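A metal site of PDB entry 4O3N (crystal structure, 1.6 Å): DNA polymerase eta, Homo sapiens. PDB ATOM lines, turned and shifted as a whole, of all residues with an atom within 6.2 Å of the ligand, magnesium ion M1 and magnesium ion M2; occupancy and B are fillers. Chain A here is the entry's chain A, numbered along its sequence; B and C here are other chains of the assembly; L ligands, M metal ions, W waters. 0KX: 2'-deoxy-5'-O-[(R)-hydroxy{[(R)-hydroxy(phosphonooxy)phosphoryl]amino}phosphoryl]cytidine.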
ATOM      1  N   ASP A  16     -22.464 -15.615 -29.606  1.00  0.00           N
ATOM      2  CA  ASP A  16     -22.343 -16.589 -28.508  1.00  0.00           C
ATOM      3  C   ASP A  16     -23.120 -17.830 -28.861  1.00  0.00           C
ATOM      4  O   ASP A  16     -24.316 -17.766 -29.128  1.00  0.00           O
ATOM      5  CB  ASP A  16     -22.861 -16.033 -27.183  1.00  0.00           C
ATOM      6  CG  ASP A  16     -22.640 -16.986 -26.056  1.00  0.00           C
ATOM      7  OD1 ASP A  16     -21.645 -16.836 -25.367  1.00  0.00           O
ATOM      8  OD2 ASP A  16     -23.429 -17.888 -25.922  1.00  0.00           O
ATOM      9  N   MET A  17     -22.468 -18.965 -28.803  1.00  0.00           N
ATOM     10  CA  MET A  17     -23.166 -20.158 -29.206  1.00  0.00           C
ATOM     11  C   MET A  17     -24.291 -20.563 -28.240  1.00  0.00           C
ATOM     12  O   MET A  17     -24.178 -20.387 -27.056  1.00  0.00           O
ATOM     13  CB  MET A  17     -22.193 -21.355 -29.290  1.00  0.00           C
ATOM     14  CG  MET A  17     -20.977 -21.066 -30.229  1.00  0.00           C
ATOM     15  SD  MET A  17     -21.355 -20.571 -31.910  1.00  0.00           S
ATOM     16  CE  MET A  17     -22.179 -21.959 -32.505  1.00  0.00           C
ATOM     17  N   ASP A  18     -25.356 -21.084 -28.801  1.00  0.00           N
ATOM     18  CA  ASP A  18     -26.477 -21.544 -27.954  1.00  0.00           C
ATOM     19  C   ASP A  18     -26.105 -22.890 -27.323  1.00  0.00           C
ATOM     20  O   ASP A  18     -25.578 -23.767 -28.026  1.00  0.00           O
ATOM     21  CB  ASP A  18     -27.775 -21.625 -28.744  1.00  0.00           C
ATOM     22  CG  ASP A  18     -28.210 -20.259 -29.318  1.00  0.00           C
ATOM     23  OD1 ASP A  18     -27.899 -19.217 -28.718  1.00  0.00           O
ATOM     24  OD2 ASP A  18     -28.879 -20.249 -30.327  1.00  0.00           O
ATOM     25  N   CYS A  19     -26.382 -23.013 -26.028  1.00  0.00           N
ATOM     26  CA  CYS A  19     -26.130 -24.223 -25.206  1.00  0.00           C
ATOM     27  C   CYS A  19     -24.992 -25.039 -25.818  1.00  0.00           C
ATOM     28  O   CYS A  19     -25.174 -26.179 -26.238  1.00  0.00           O
ATOM     29  CB  CYS A  19     -27.396 -25.079 -25.024  1.00  0.00           C
ATOM     30  SG  CYS A  19     -28.348 -25.550 -26.491  1.00  0.00           S
ATOM     31  N   PHE A  20     -23.800 -24.437 -25.843  1.00  0.00           N
ATOM     32  CA  PHE A  20     -22.770 -24.904 -26.782  1.00  0.00           C
ATOM     33  C   PHE A  20     -22.398 -26.379 -26.608  1.00  0.00           C
ATOM     34  O   PHE A  20     -22.440 -27.095 -27.580  1.00  0.00           O
ATOM     35  CB  PHE A  20     -21.525 -24.057 -26.635  1.00  0.00           C
ATOM     36  CG  PHE A  20     -20.455 -24.364 -27.646  1.00  0.00           C
ATOM     37  CD1 PHE A  20     -20.768 -24.595 -28.982  1.00  0.00           C
ATOM     38  CD2 PHE A  20     -19.137 -24.502 -27.239  1.00  0.00           C
ATOM     39  CE1 PHE A  20     -19.781 -24.876 -29.927  1.00  0.00           C
ATOM     40  CE2 PHE A  20     -18.116 -24.797 -28.211  1.00  0.00           C
ATOM     41  CZ  PHE A  20     -18.479 -24.986 -29.517  1.00  0.00           C
ATOM     42  N   PHE A  21     -22.012 -26.803 -25.401  1.00  0.00           N
ATOM     43  CA  PHE A  21     -21.521 -28.187 -25.278  1.00  0.00           C
ATOM     44  C   PHE A  21     -22.656 -29.167 -25.574  1.00  0.00           C
ATOM     45  O   PHE A  21     -22.410 -30.193 -26.158  1.00  0.00           O
ATOM     46  CB  PHE A  21     -20.962 -28.530 -23.898  1.00  0.00           C
ATOM     47  CG  PHE A  21     -19.670 -27.866 -23.556  1.00  0.00           C
ATOM     48  CD1 PHE A  21     -19.144 -26.812 -24.323  1.00  0.00           C
ATOM     49  CD2 PHE A  21     -18.998 -28.267 -22.408  1.00  0.00           C
ATOM     50  CE1 PHE A  21     -17.908 -26.224 -23.960  1.00  0.00           C
ATOM     51  CE2 PHE A  21     -17.748 -27.718 -22.055  1.00  0.00           C
ATOM     52  CZ  PHE A  21     -17.232 -26.639 -22.848  1.00  0.00           C
ATOM     53  N   VAL A  22     -23.900 -28.806 -25.259  1.00  0.00           N
ATOM     54  CA  VAL A  22     -25.037 -29.650 -25.643  1.00  0.00           C
ATOM     55  C   VAL A  22     -25.111 -29.742 -27.179  1.00  0.00           C
ATOM     56  O   VAL A  22     -25.317 -30.829 -27.710  1.00  0.00           O
ATOM     57  CB  VAL A  22     -26.310 -29.116 -25.046  1.00  0.00           C
ATOM     58  CG1 VAL A  22     -27.569 -29.747 -25.710  1.00  0.00           C
ATOM     59  CG2 VAL A  22     -26.315 -29.334 -23.540  1.00  0.00           C
ATOM     60  N   ILE A  51     -22.837 -29.191 -16.676  1.00  0.00           N
ATOM     61  CA  ILE A  51     -22.099 -27.973 -17.115  1.00  0.00           C
ATOM     62  C   ILE A  51     -22.766 -27.318 -18.340  1.00  0.00           C
ATOM     63  O   ILE A  51     -22.403 -26.188 -18.692  1.00  0.00           O
ATOM     64  CB  ILE A  51     -20.659 -28.254 -17.405  1.00  0.00           C
ATOM     65  CG1 ILE A  51     -20.458 -29.180 -18.607  1.00  0.00           C
ATOM     66  CG2 ILE A  51     -19.965 -28.744 -16.088  1.00  0.00           C
ATOM     67  CD1 ILE A  51     -18.994 -29.404 -18.917  1.00  0.00           C
ATOM     68  N   ALA A  52     -23.775 -27.942 -18.940  1.00  0.00           N
ATOM     69  CA  ALA A  52     -24.520 -27.285 -20.046  1.00  0.00           C
ATOM     70  C   ALA A  52     -25.876 -27.919 -20.165  1.00  0.00           C
ATOM     71  O   ALA A  52     -26.004 -29.130 -19.908  1.00  0.00           O
ATOM     72  CB  ALA A  52     -23.733 -27.400 -21.401  1.00  0.00           C
ATOM     73  N   VAL A  53     -26.884 -27.131 -20.604  1.00  0.00           N
ATOM     74  CA  VAL A  53     -28.270 -27.531 -20.532  1.00  0.00           C
ATOM     75  C   VAL A  53     -29.003 -27.107 -21.782  1.00  0.00           C
ATOM     76  O   VAL A  53     -28.979 -25.895 -22.120  1.00  0.00           O
ATOM     77  CB  VAL A  53     -28.956 -26.875 -19.279  1.00  0.00           C
ATOM     78  CG1 VAL A  53     -30.347 -27.487 -19.044  1.00  0.00           C
ATOM     79  CG2 VAL A  53     -28.096 -27.087 -18.049  1.00  0.00           C
ATOM     80  N   TYR A  55     -32.205 -25.992 -24.180  1.00  0.00           N
ATOM     81  CA  TYR A  55     -33.348 -25.148 -23.840  1.00  0.00           C
ATOM     82  C   TYR A  55     -34.565 -25.955 -23.460  1.00  0.00           C
ATOM     83  O   TYR A  55     -35.267 -25.502 -22.548  1.00  0.00           O
ATOM     84  CB  TYR A  55     -33.644 -24.136 -24.987  1.00  0.00           C
ATOM     85  CG  TYR A  55     -32.641 -23.007 -24.968  1.00  0.00           C
ATOM     86  CD1 TYR A  55     -31.365 -23.177 -25.505  1.00  0.00           C
ATOM     87  CD2 TYR A  55     -32.903 -21.827 -24.288  1.00  0.00           C
ATOM     88  CE1 TYR A  55     -30.404 -22.174 -25.387  1.00  0.00           C
ATOM     89  CE2 TYR A  55     -31.953 -20.825 -24.151  1.00  0.00           C
ATOM     90  CZ  TYR A  55     -30.709 -20.975 -24.710  1.00  0.00           C
ATOM     91  OH  TYR A  55     -29.768 -19.961 -24.619  1.00  0.00           O
ATOM     92  N   ARG A  58     -33.991 -26.584 -19.803  1.00  0.00           N
ATOM     93  CA  ARG A  58     -34.132 -25.343 -18.996  1.00  0.00           C
ATOM     94  C   ARG A  58     -35.607 -25.082 -18.619  1.00  0.00           C
ATOM     95  O   ARG A  58     -35.848 -24.506 -17.529  1.00  0.00           O
ATOM     96  CB  ARG A  58     -33.574 -24.120 -19.737  1.00  0.00           C
ATOM     97  CG  ARG A  58     -32.115 -24.244 -19.988  1.00  0.00           C
ATOM     98  CD  ARG A  58     -31.541 -23.027 -20.725  1.00  0.00           C
ATOM     99  NE  ARG A  58     -30.230 -23.380 -21.302  1.00  0.00           N
ATOM    100  CZ  ARG A  58     -29.325 -22.511 -21.727  1.00  0.00           C
ATOM    101  NH1 ARG A  58     -29.570 -21.200 -21.652  1.00  0.00           N
ATOM    102  NH2 ARG A  58     -28.165 -22.983 -22.236  1.00  0.00           N
ATOM    103  N   ARG A  64     -27.102 -25.262 -14.942  1.00  0.00           N
ATOM    104  CA  ARG A  64     -25.714 -25.541 -14.656  1.00  0.00           C
ATOM    105  C   ARG A  64     -25.464 -25.603 -13.158  1.00  0.00           C
ATOM    106  O   ARG A  64     -26.157 -24.939 -12.350  1.00  0.00           O
ATOM    107  CB  ARG A  64     -24.814 -24.494 -15.324  1.00  0.00           C
ATOM    108  CG  ARG A  64     -23.369 -24.615 -15.085  1.00  0.00           C
ATOM    109  CD  ARG A  64     -22.715 -23.286 -15.432  1.00  0.00           C
ATOM    110  NE  ARG A  64     -23.089 -22.863 -16.767  1.00  0.00           N
ATOM    111  CZ  ARG A  64     -23.657 -21.691 -17.070  1.00  0.00           C
ATOM    112  NH1 ARG A  64     -23.940 -20.780 -16.140  1.00  0.00           N
ATOM    113  NH2 ARG A  64     -23.916 -21.429 -18.356  1.00  0.00           N
ATOM    114  N   LEU A  92     -11.567 -31.711 -22.125  1.00  0.00           N
ATOM    115  CA  LEU A  92     -12.481 -30.841 -22.888  1.00  0.00           C
ATOM    116  C   LEU A  92     -12.117 -30.696 -24.375  1.00  0.00           C
ATOM    117  O   LEU A  92     -12.656 -29.814 -25.069  1.00  0.00           O
ATOM    118  CB  LEU A  92     -12.523 -29.471 -22.205  1.00  0.00           C
ATOM    119  CG  LEU A  92     -13.005 -29.532 -20.779  1.00  0.00           C
ATOM    120  CD1 LEU A  92     -12.804 -28.154 -20.258  1.00  0.00           C
ATOM    121  CD2 LEU A  92     -14.506 -29.952 -20.775  1.00  0.00           C
ATOM    122  N   SER A 116     -14.270 -16.460 -25.142  1.00  0.00           N
ATOM    123  CA  SER A 116     -14.444 -17.683 -24.358  1.00  0.00           C
ATOM    124  C   SER A 116     -14.419 -18.851 -25.333  1.00  0.00           C
ATOM    125  O   SER A 116     -14.309 -18.671 -26.531  1.00  0.00           O
ATOM    126  CB  SER A 116     -15.781 -17.704 -23.607  1.00  0.00           C
ATOM    127  OG  SER A 116     -16.905 -18.017 -24.483  1.00  0.00           O
ATOM    128  N   ILE A 117     -14.668 -20.065 -24.820  1.00  0.00           N
ATOM    129  CA  ILE A 117     -14.723 -21.209 -25.742  1.00  0.00           C
ATOM    130  C   ILE A 117     -15.879 -21.100 -26.772  1.00  0.00           C
ATOM    131  O   ILE A 117     -15.830 -21.728 -27.837  1.00  0.00           O
ATOM    132  CB  ILE A 117     -14.811 -22.529 -24.933  1.00  0.00           C
ATOM    133  CG1 ILE A 117     -14.421 -23.715 -25.788  1.00  0.00           C
ATOM    134  CG2 ILE A 117     -16.227 -22.706 -24.328  1.00  0.00           C
ATOM    135  CD1 ILE A 117     -14.178 -24.962 -24.901  1.00  0.00           C
ATOM    136  N   ASP A 118     -16.904 -20.295 -26.432  1.00  0.00           N
ATOM    137  CA  ASP A 118     -18.055 -20.273 -27.318  1.00  0.00           C
ATOM    138  C   ASP A 118     -18.480 -18.874 -27.739  1.00  0.00           C
ATOM    139  O   ASP A 118     -19.583 -18.720 -28.258  1.00  0.00           O
ATOM    140  CB  ASP A 118     -19.248 -21.045 -26.709  1.00  0.00           C
ATOM    141  CG  ASP A 118     -20.175 -20.149 -25.851  1.00  0.00           C
ATOM    142  OD1 ASP A 118     -19.685 -19.247 -25.101  1.00  0.00           O
ATOM    143  OD2 ASP A 118     -21.411 -20.288 -26.058  1.00  0.00           O
ATOM    144  N   GLU A 119     -17.609 -17.881 -27.575  1.00  0.00           N
ATOM    145  CA  GLU A 119     -17.987 -16.553 -28.077  1.00  0.00           C
ATOM    146  C   GLU A 119     -16.844 -15.721 -28.503  1.00  0.00           C
ATOM    147  O   GLU A 119     -15.689 -15.934 -28.070  1.00  0.00           O
ATOM    148  CB  GLU A 119     -18.779 -15.779 -27.072  1.00  0.00           C
ATOM    149  CG  GLU A 119     -18.032 -15.337 -25.882  1.00  0.00           C
ATOM    150  CD  GLU A 119     -18.927 -15.299 -24.656  1.00  0.00           C
ATOM    151  OE1 GLU A 119     -19.203 -16.367 -24.086  1.00  0.00           O
ATOM    152  OE2 GLU A 119     -19.398 -14.203 -24.258  1.00  0.00           O
ATOM    153  N   LYS A 227     -22.641  -7.558 -25.878  1.00  0.00           N
ATOM    154  CA  LYS A 227     -22.796  -8.728 -25.049  1.00  0.00           C
ATOM    155  C   LYS A 227     -24.177  -8.732 -24.396  1.00  0.00           C
ATOM    156  O   LYS A 227     -24.851  -9.751 -24.383  1.00  0.00           O
ATOM    157  CB  LYS A 227     -21.701  -8.783 -23.949  1.00  0.00           C
ATOM    158  CG  LYS A 227     -21.851  -9.932 -22.960  1.00  0.00           C
ATOM    159  CD  LYS A 227     -21.756 -11.323 -23.682  1.00  0.00           C
ATOM    160  CE  LYS A 227     -21.591 -12.441 -22.580  1.00  0.00           C
ATOM    161  NZ  LYS A 227     -21.794 -13.894 -22.944  1.00  0.00           N
ATOM    162  N   LYS A 234     -31.807 -14.659 -26.953  1.00  0.00           N
ATOM    163  CA  LYS A 234     -31.280 -16.012 -27.092  1.00  0.00           C
ATOM    164  C   LYS A 234     -32.446 -16.975 -26.830  1.00  0.00           C
ATOM    165  O   LYS A 234     -33.248 -16.696 -25.901  1.00  0.00           O
ATOM    166  CB  LYS A 234     -30.158 -16.161 -26.053  1.00  0.00           C
ATOM    167  CG  LYS A 234     -29.038 -17.015 -26.340  1.00  0.00           C
ATOM    168  CD  LYS A 234     -28.019 -16.937 -25.257  1.00  0.00           C
ATOM    169  CE  LYS A 234     -26.628 -16.846 -25.906  1.00  0.00           C
ATOM    170  NZ  LYS A 234     -26.272 -18.102 -26.742  1.00  0.00           N
ATOM    171  N   PRO A 235     -32.542 -18.135 -27.527  1.00  0.00           N
ATOM    172  CA  PRO A 235     -31.549 -18.667 -28.485  1.00  0.00           C
ATOM    173  C   PRO A 235     -31.931 -18.399 -29.952  1.00  0.00           C
ATOM    174  O   PRO A 235     -33.092 -18.073 -30.305  1.00  0.00           O
ATOM    175  CB  PRO A 235     -31.575 -20.183 -28.225  1.00  0.00           C
ATOM    176  CG  PRO A 235     -33.101 -20.466 -27.981  1.00  0.00           C
ATOM    177  CD  PRO A 235     -33.583 -19.153 -27.241  1.00  0.00           C
ATOM    178  P    DT B   8     -19.994 -14.694 -18.245  1.00  0.00           P
ATOM    179  OP1  DT B   8     -20.855 -14.004 -19.240  1.00  0.00           O
ATOM    180  OP2  DT B   8     -20.520 -15.245 -16.961  1.00  0.00           O
ATOM    181  O5'  DT B   8     -19.251 -15.900 -18.982  1.00  0.00           O
ATOM    182  C5'  DT B   8     -18.645 -15.708 -20.221  1.00  0.00           C
ATOM    183  C4'  DT B   8     -18.177 -17.043 -20.679  1.00  0.00           C
ATOM    184  O4'  DT B   8     -17.376 -17.585 -19.618  1.00  0.00           O
ATOM    185  C3'  DT B   8     -19.316 -18.040 -20.932  1.00  0.00           C
ATOM    186  O3'  DT B   8     -19.100 -18.677 -22.205  1.00  0.00           O
ATOM    187  C2'  DT B   8     -19.222 -19.011 -19.745  1.00  0.00           C
ATOM    188  C1'  DT B   8     -17.767 -18.923 -19.356  1.00  0.00           C
ATOM    189  N1   DT B   8     -17.526 -19.183 -17.915  1.00  0.00           N
ATOM    190  C2   DT B   8     -16.732 -20.251 -17.552  1.00  0.00           C
ATOM    191  O2   DT B   8     -16.254 -21.019 -18.366  1.00  0.00           O
ATOM    192  N3   DT B   8     -16.540 -20.389 -16.201  1.00  0.00           N
ATOM    193  C4   DT B   8     -17.077 -19.596 -15.212  1.00  0.00           C
ATOM    194  O4   DT B   8     -16.872 -19.791 -14.022  1.00  0.00           O
ATOM    195  C5   DT B   8     -17.918 -18.520 -15.659  1.00  0.00           C
ATOM    196  C7   DT B   8     -18.529 -17.590 -14.665  1.00  0.00           C
ATOM    197  C6   DT B   8     -18.092 -18.362 -16.978  1.00  0.00           C
ATOM    198  P    DT C   3     -20.779 -28.139  -3.433  1.00  0.00           P
ATOM    199  OP1  DT C   3     -20.285 -27.249  -2.354  1.00  0.00           O
ATOM    200  OP2  DT C   3     -22.220 -28.446  -3.669  1.00  0.00           O
ATOM    201  O5'  DT C   3     -20.169 -27.516  -4.753  1.00  0.00           O
ATOM    202  C5'  DT C   3     -20.948 -27.474  -5.933  1.00  0.00           C
ATOM    203  C4'  DT C   3     -20.195 -28.204  -7.000  1.00  0.00           C
ATOM    204  O4'  DT C   3     -20.780 -27.953  -8.301  1.00  0.00           O
ATOM    205  C3'  DT C   3     -18.719 -27.785  -7.132  1.00  0.00           C
ATOM    206  O3'  DT C   3     -17.897 -28.870  -6.879  1.00  0.00           O
ATOM    207  C2'  DT C   3     -18.579 -27.356  -8.591  1.00  0.00           C
ATOM    208  C1'  DT C   3     -19.704 -28.161  -9.200  1.00  0.00           C
ATOM    209  N1   DT C   3     -20.082 -27.695 -10.510  1.00  0.00           N
ATOM    210  C2   DT C   3     -20.050 -28.589 -11.571  1.00  0.00           C
ATOM    211  O2   DT C   3     -19.765 -29.801 -11.446  1.00  0.00           O
ATOM    212  N3   DT C   3     -20.377 -28.039 -12.743  1.00  0.00           N
ATOM    213  C4   DT C   3     -20.708 -26.697 -12.987  1.00  0.00           C
ATOM    214  O4   DT C   3     -20.996 -26.287 -14.106  1.00  0.00           O
ATOM    215  C5   DT C   3     -20.689 -25.822 -11.855  1.00  0.00           C
ATOM    216  C7   DT C   3     -21.029 -24.358 -12.021  1.00  0.00           C
ATOM    217  C6   DT C   3     -20.375 -26.354 -10.680  1.00  0.00           C
ATOM    218  P    DG C   4     -16.334 -28.714  -7.143  1.00  0.00           P
ATOM    219  OP1  DG C   4     -15.651 -29.867  -6.518  1.00  0.00           O
ATOM    220  OP2  DG C   4     -16.000 -27.278  -7.061  1.00  0.00           O
ATOM    221  O5'  DG C   4     -16.162 -28.969  -8.709  1.00  0.00           O
ATOM    222  C5'  DG C   4     -16.278 -30.241  -9.253  1.00  0.00           C
ATOM    223  C4'  DG C   4     -15.614 -30.216 -10.621  1.00  0.00           C
ATOM    224  O4'  DG C   4     -16.221 -29.209 -11.505  1.00  0.00           O
ATOM    225  C3'  DG C   4     -14.142 -29.886 -10.605  1.00  0.00           C
ATOM    226  O3'  DG C   4     -13.555 -30.650 -11.656  1.00  0.00           O
ATOM    227  C2'  DG C   4     -14.105 -28.390 -10.890  1.00  0.00           C
ATOM    228  C1'  DG C   4     -15.248 -28.277 -11.917  1.00  0.00           C
ATOM    229  N9   DG C   4     -15.912 -27.001 -11.914  1.00  0.00           N
ATOM    230  C8   DG C   4     -16.183 -26.139 -10.891  1.00  0.00           C
ATOM    231  N7   DG C   4     -16.868 -25.072 -11.272  1.00  0.00           N
ATOM    232  C5   DG C   4     -17.044 -25.279 -12.651  1.00  0.00           C
ATOM    233  C6   DG C   4     -17.721 -24.510 -13.602  1.00  0.00           C
ATOM    234  O6   DG C   4     -18.264 -23.401 -13.453  1.00  0.00           O
ATOM    235  N1   DG C   4     -17.669 -25.109 -14.871  1.00  0.00           N
ATOM    236  C2   DG C   4     -17.058 -26.310 -15.167  1.00  0.00           C
ATOM    237  N2   DG C   4     -17.082 -26.715 -16.471  1.00  0.00           N
ATOM    238  N3   DG C   4     -16.431 -27.058 -14.264  1.00  0.00           N
ATOM    239  C4   DG C   4     -16.500 -26.478 -13.027  1.00  0.00           C
ATOM    240  P    DA C   5     -12.004 -30.636 -12.017  1.00  0.00           P
ATOM    241  OP1  DA C   5     -11.602 -32.014 -12.241  1.00  0.00           O
ATOM    242  OP2  DA C   5     -11.283 -29.824 -11.006  1.00  0.00           O
ATOM    243  O5'  DA C   5     -11.926 -29.749 -13.356  1.00  0.00           O
ATOM    244  C5'  DA C   5     -12.425 -30.299 -14.556  1.00  0.00           C
ATOM    245  C4'  DA C   5     -12.173 -29.337 -15.686  1.00  0.00           C
ATOM    246  O4'  DA C   5     -13.021 -28.184 -15.485  1.00  0.00           O
ATOM    247  C3'  DA C   5     -10.749 -28.828 -15.813  1.00  0.00           C
ATOM    248  O3'  DA C   5     -10.451 -28.689 -17.198  1.00  0.00           O
ATOM    249  C2'  DA C   5     -10.818 -27.436 -15.144  1.00  0.00           C
ATOM    250  C1'  DA C   5     -12.242 -27.009 -15.585  1.00  0.00           C
ATOM    251  N9   DA C   5     -12.862 -25.978 -14.773  1.00  0.00           N
ATOM    252  C8   DA C   5     -12.781 -25.821 -13.406  1.00  0.00           C
ATOM    253  N7   DA C   5     -13.414 -24.775 -12.954  1.00  0.00           N
ATOM    254  C5   DA C   5     -14.008 -24.224 -14.085  1.00  0.00           C
ATOM    255  C6   DA C   5     -14.756 -23.067 -14.261  1.00  0.00           C
ATOM    256  N6   DA C   5     -15.131 -22.256 -13.244  1.00  0.00           N
ATOM    257  N1   DA C   5     -15.139 -22.785 -15.525  1.00  0.00           N
ATOM    258  C2   DA C   5     -14.735 -23.576 -16.529  1.00  0.00           C
ATOM    259  N3   DA C   5     -14.002 -24.669 -16.484  1.00  0.00           N
ATOM    260  C4   DA C   5     -13.643 -24.926 -15.212  1.00  0.00           C
HETATM  261  PG  0KX L   1     -26.361 -20.188 -23.771  1.00  0.00           P
HETATM  262  O1G 0KX L   1     -25.156 -19.390 -24.189  1.00  0.00           O
HETATM  263  O2G 0KX L   1     -27.078 -19.556 -22.552  1.00  0.00           O
HETATM  264  O3G 0KX L   1     -27.286 -20.504 -24.877  1.00  0.00           O
HETATM  265  PB  0KX L   1     -24.229 -22.066 -23.140  1.00  0.00           P
HETATM  266  O1B 0KX L   1     -23.530 -21.804 -24.456  1.00  0.00           O
HETATM  267  O2B 0KX L   1     -24.257 -23.494 -22.674  1.00  0.00           O
HETATM  268  O3B 0KX L   1     -25.752 -21.616 -23.248  1.00  0.00           O
HETATM  269  PA  0KX L   1     -22.256 -20.128 -22.032  1.00  0.00           P
HETATM  270  O1A 0KX L   1     -22.201 -19.367 -20.719  1.00  0.00           O
HETATM  271  O2A 0KX L   1     -22.157 -19.337 -23.259  1.00  0.00           O
HETATM  272  N3A 0KX L   1     -23.642 -21.089 -21.914  1.00  0.00           N
HETATM  273  O5' 0KX L   1     -21.040 -21.148 -21.918  1.00  0.00           O
HETATM  274  C5' 0KX L   1     -20.530 -21.872 -23.054  1.00  0.00           C
HETATM  275  C4' 0KX L   1     -20.125 -23.232 -22.705  1.00  0.00           C
HETATM  276  O4' 0KX L   1     -19.010 -23.130 -21.653  1.00  0.00           O
HETATM  277  C3' 0KX L   1     -21.159 -24.124 -21.989  1.00  0.00           C
HETATM  278  O3' 0KX L   1     -21.965 -24.843 -22.988  1.00  0.00           O
HETATM  279  C2' 0KX L   1     -20.402 -24.994 -21.203  1.00  0.00           C
HETATM  280  C1' 0KX L   1     -19.126 -24.133 -20.752  1.00  0.00           C
HETATM  281  N1  0KX L   1     -19.293 -23.573 -19.448  1.00  0.00           N
HETATM  282  C2  0KX L   1     -18.624 -24.226 -18.382  1.00  0.00           C
HETATM  283  N3  0KX L   1     -18.735 -23.612 -17.106  1.00  0.00           N
HETATM  284  C4  0KX L   1     -19.471 -22.458 -16.901  1.00  0.00           C
HETATM  285  C5  0KX L   1     -20.105 -21.777 -17.997  1.00  0.00           C
HETATM  286  C6  0KX L   1     -19.988 -22.381 -19.280  1.00  0.00           C
HETATM  287  O2  0KX L   1     -18.018 -25.312 -18.576  1.00  0.00           O
HETATM  288  N4  0KX L   1     -19.510 -21.924 -15.596  1.00  0.00           N
HETATM  289 MG    MG M   1     -23.256 -19.786 -25.138  1.00  0.00          MG
HETATM  290 MG    MG M   2     -20.674 -17.788 -23.852  1.00  0.00          MG
HETATM  291  O   HOH W   1     -24.648 -16.926 -23.043  1.00  0.00           O
HETATM  292  O   HOH W   2     -26.248 -20.139 -20.081  1.00  0.00           O
HETATM  293  O   HOH W   3     -21.439 -19.713 -15.423  1.00  0.00           O
HETATM  294  O   HOH W   4     -15.963 -22.788 -20.438  1.00  0.00           O
HETATM  295  O   HOH W   5     -16.028 -26.640 -19.388  1.00  0.00           O
HETATM  296  O   HOH W   6     -25.958 -24.438 -20.893  1.00  0.00           O
HETATM  297  O   HOH W   7     -21.958 -16.745 -22.481  1.00  0.00           O
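The side-chain amino group of Lys 234 lies within salt-bridge range of an oxygen (O3G) of the ligand, 3.2 Å away. The guanidinium group (NH2) of Arg 64 is in salt-bridge range of an oxygen (O1A) of the ligand (3.6 Å). N of Phe 21 sits at hydrogen-bond distance from O3' of the ligand, at 3.1 Å. N of Phe 20 lies within hydrogen-bond range of O2B of the ligand (3.3 Å). NH1 of Arg 58 lies within salt-bridge range of O2G of the ligand (3.1 Å). O6 of DG 4 of chain C is in hydrogen-bond range of a nitrogen (N4) of the ligand (2.9 Å). N of Cys 19 sits at hydrogen-bond distance from O3G of the ligand, 2.9 Å away. N3 of DT 8 of chain B sits close to a nitrogen (N4) of the ligand (3.4 Å). The side-chain hydroxyl (OH) of Tyr 55 is in hydrogen-bond range of an oxygen (O3G) of the ligand, at 2.6 Å.
The side-chain carboxylate (OD1) of Asp 16 lies close to the side-chain amino group (NZ) of Lys 227 (3.8 Å). The backbone NH (N) of Asp 118 is in hydrogen-bond range of the side-chain hydroxyl (OG) of Ser 116. The side-chain hydroxyl (OH) of Tyr 55 sits at hydrogen-bond distance from the guanidinium group (NH1) of Arg 58 (3.2 Å). O of Asp 16 lies within hydrogen-bond range of NZ of Lys 234, 3.1 Å away. O3' of DT 8 of chain B lies close to the side-chain hydroxyl of Ser 116 (3.2 Å). OD1 of Asp 18 is in salt-bridge range of NZ of Lys 234, 2.8 Å away. The side-chain amino group (NZ) of Lys 234 sits close to the backbone carbonyl oxygen (O) of Met 17 (3.1 Å). The side-chain amino group of Lys 227 is in salt-bridge range of OP1 of DT 8 of chain B.
Merely in contact with the ligand: Asp 18, Ile 51, Ala 52 and Ile 117. Hydrophobic or aromatic side chains that line the ligand: Phe 20, Phe 21, Ala 52, Tyr 55 and Ile 117. 16 residues have an atom within 4 Å of the ligand: Asp 16, Met 17, Asp 18, Cys 19, Phe 20, Phe 21, Ile 51, Ala 52, Tyr 55, Arg 58, Arg 64, Ile 117, Asp 118, Lys 234, DT 8 of chain B and DG 4 of chain C.
Merely in contact with magnesium ion M1: Lys 234 (3.8 Å). Of the 25 residues printed, 4 come within 4 Å of magnesium ion M1. Along chain A the residues within 4 Å of magnesium ion M1 span positions 16 to 234. The nearest printed residue that does not touch magnesium ion M1 is Asp 18 (4.4 Å).
Merely in contact with magnesium ion M2: Ser 116 (3.8 Å). Within 4 Å of magnesium ion M2: Asp 16, Ser 116, Asp 118, Glu 119 and DT 8 of chain B.
Magnesium ion M1 is bound by OD2 of Asp 16 (2.1 Å), OD2 of Asp 118 (2.1 Å), O1B of the ligand (2.1 Å), O1G of the ligand (2.2 Å), O of Met 17 (2.2 Å) and O2A of the ligand (2.2 Å). Magnesium ion M1 has six donor atoms within binding distance.
Magnesium ion M2 is bound by the side-chain carboxylate of Asp 16 (2.0 Å), the side-chain carboxylate of Glu 119 (2.1 Å), water W7 (2.1 Å), the side-chain carboxylate of Asp 118 (2.2 Å), an oxygen (O2A) of the ligand (2.2 Å) and O3' of DT 8 of chain B (2.4 Å).
Water W7 bridges NZ of Lys 227 (2.9 Å) and O1A of the ligand (3.2 Å). Water W5 lies within hydrogen-bond range of an oxygen (O2) of the ligand and N2 of DG 4 of chain C. Water W6 lies within hydrogen-bond range of O2B of the ligand (2.6 Å), N of Val 53 (2.9 Å) and NH2 of Arg 58 (3.0 Å). Water W2 lies within hydrogen-bond range of O2G of the ligand and NH2 of Arg 64. Water W3 lies within hydrogen-bond range of the guanidinium group of Arg 64 (2.8 Å) and a nitrogen (N4) of the ligand (2.9 Å). Water W4 lies within hydrogen-bond range of O2 of DT 8 of chain B and an oxygen (O4') of the ligand.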
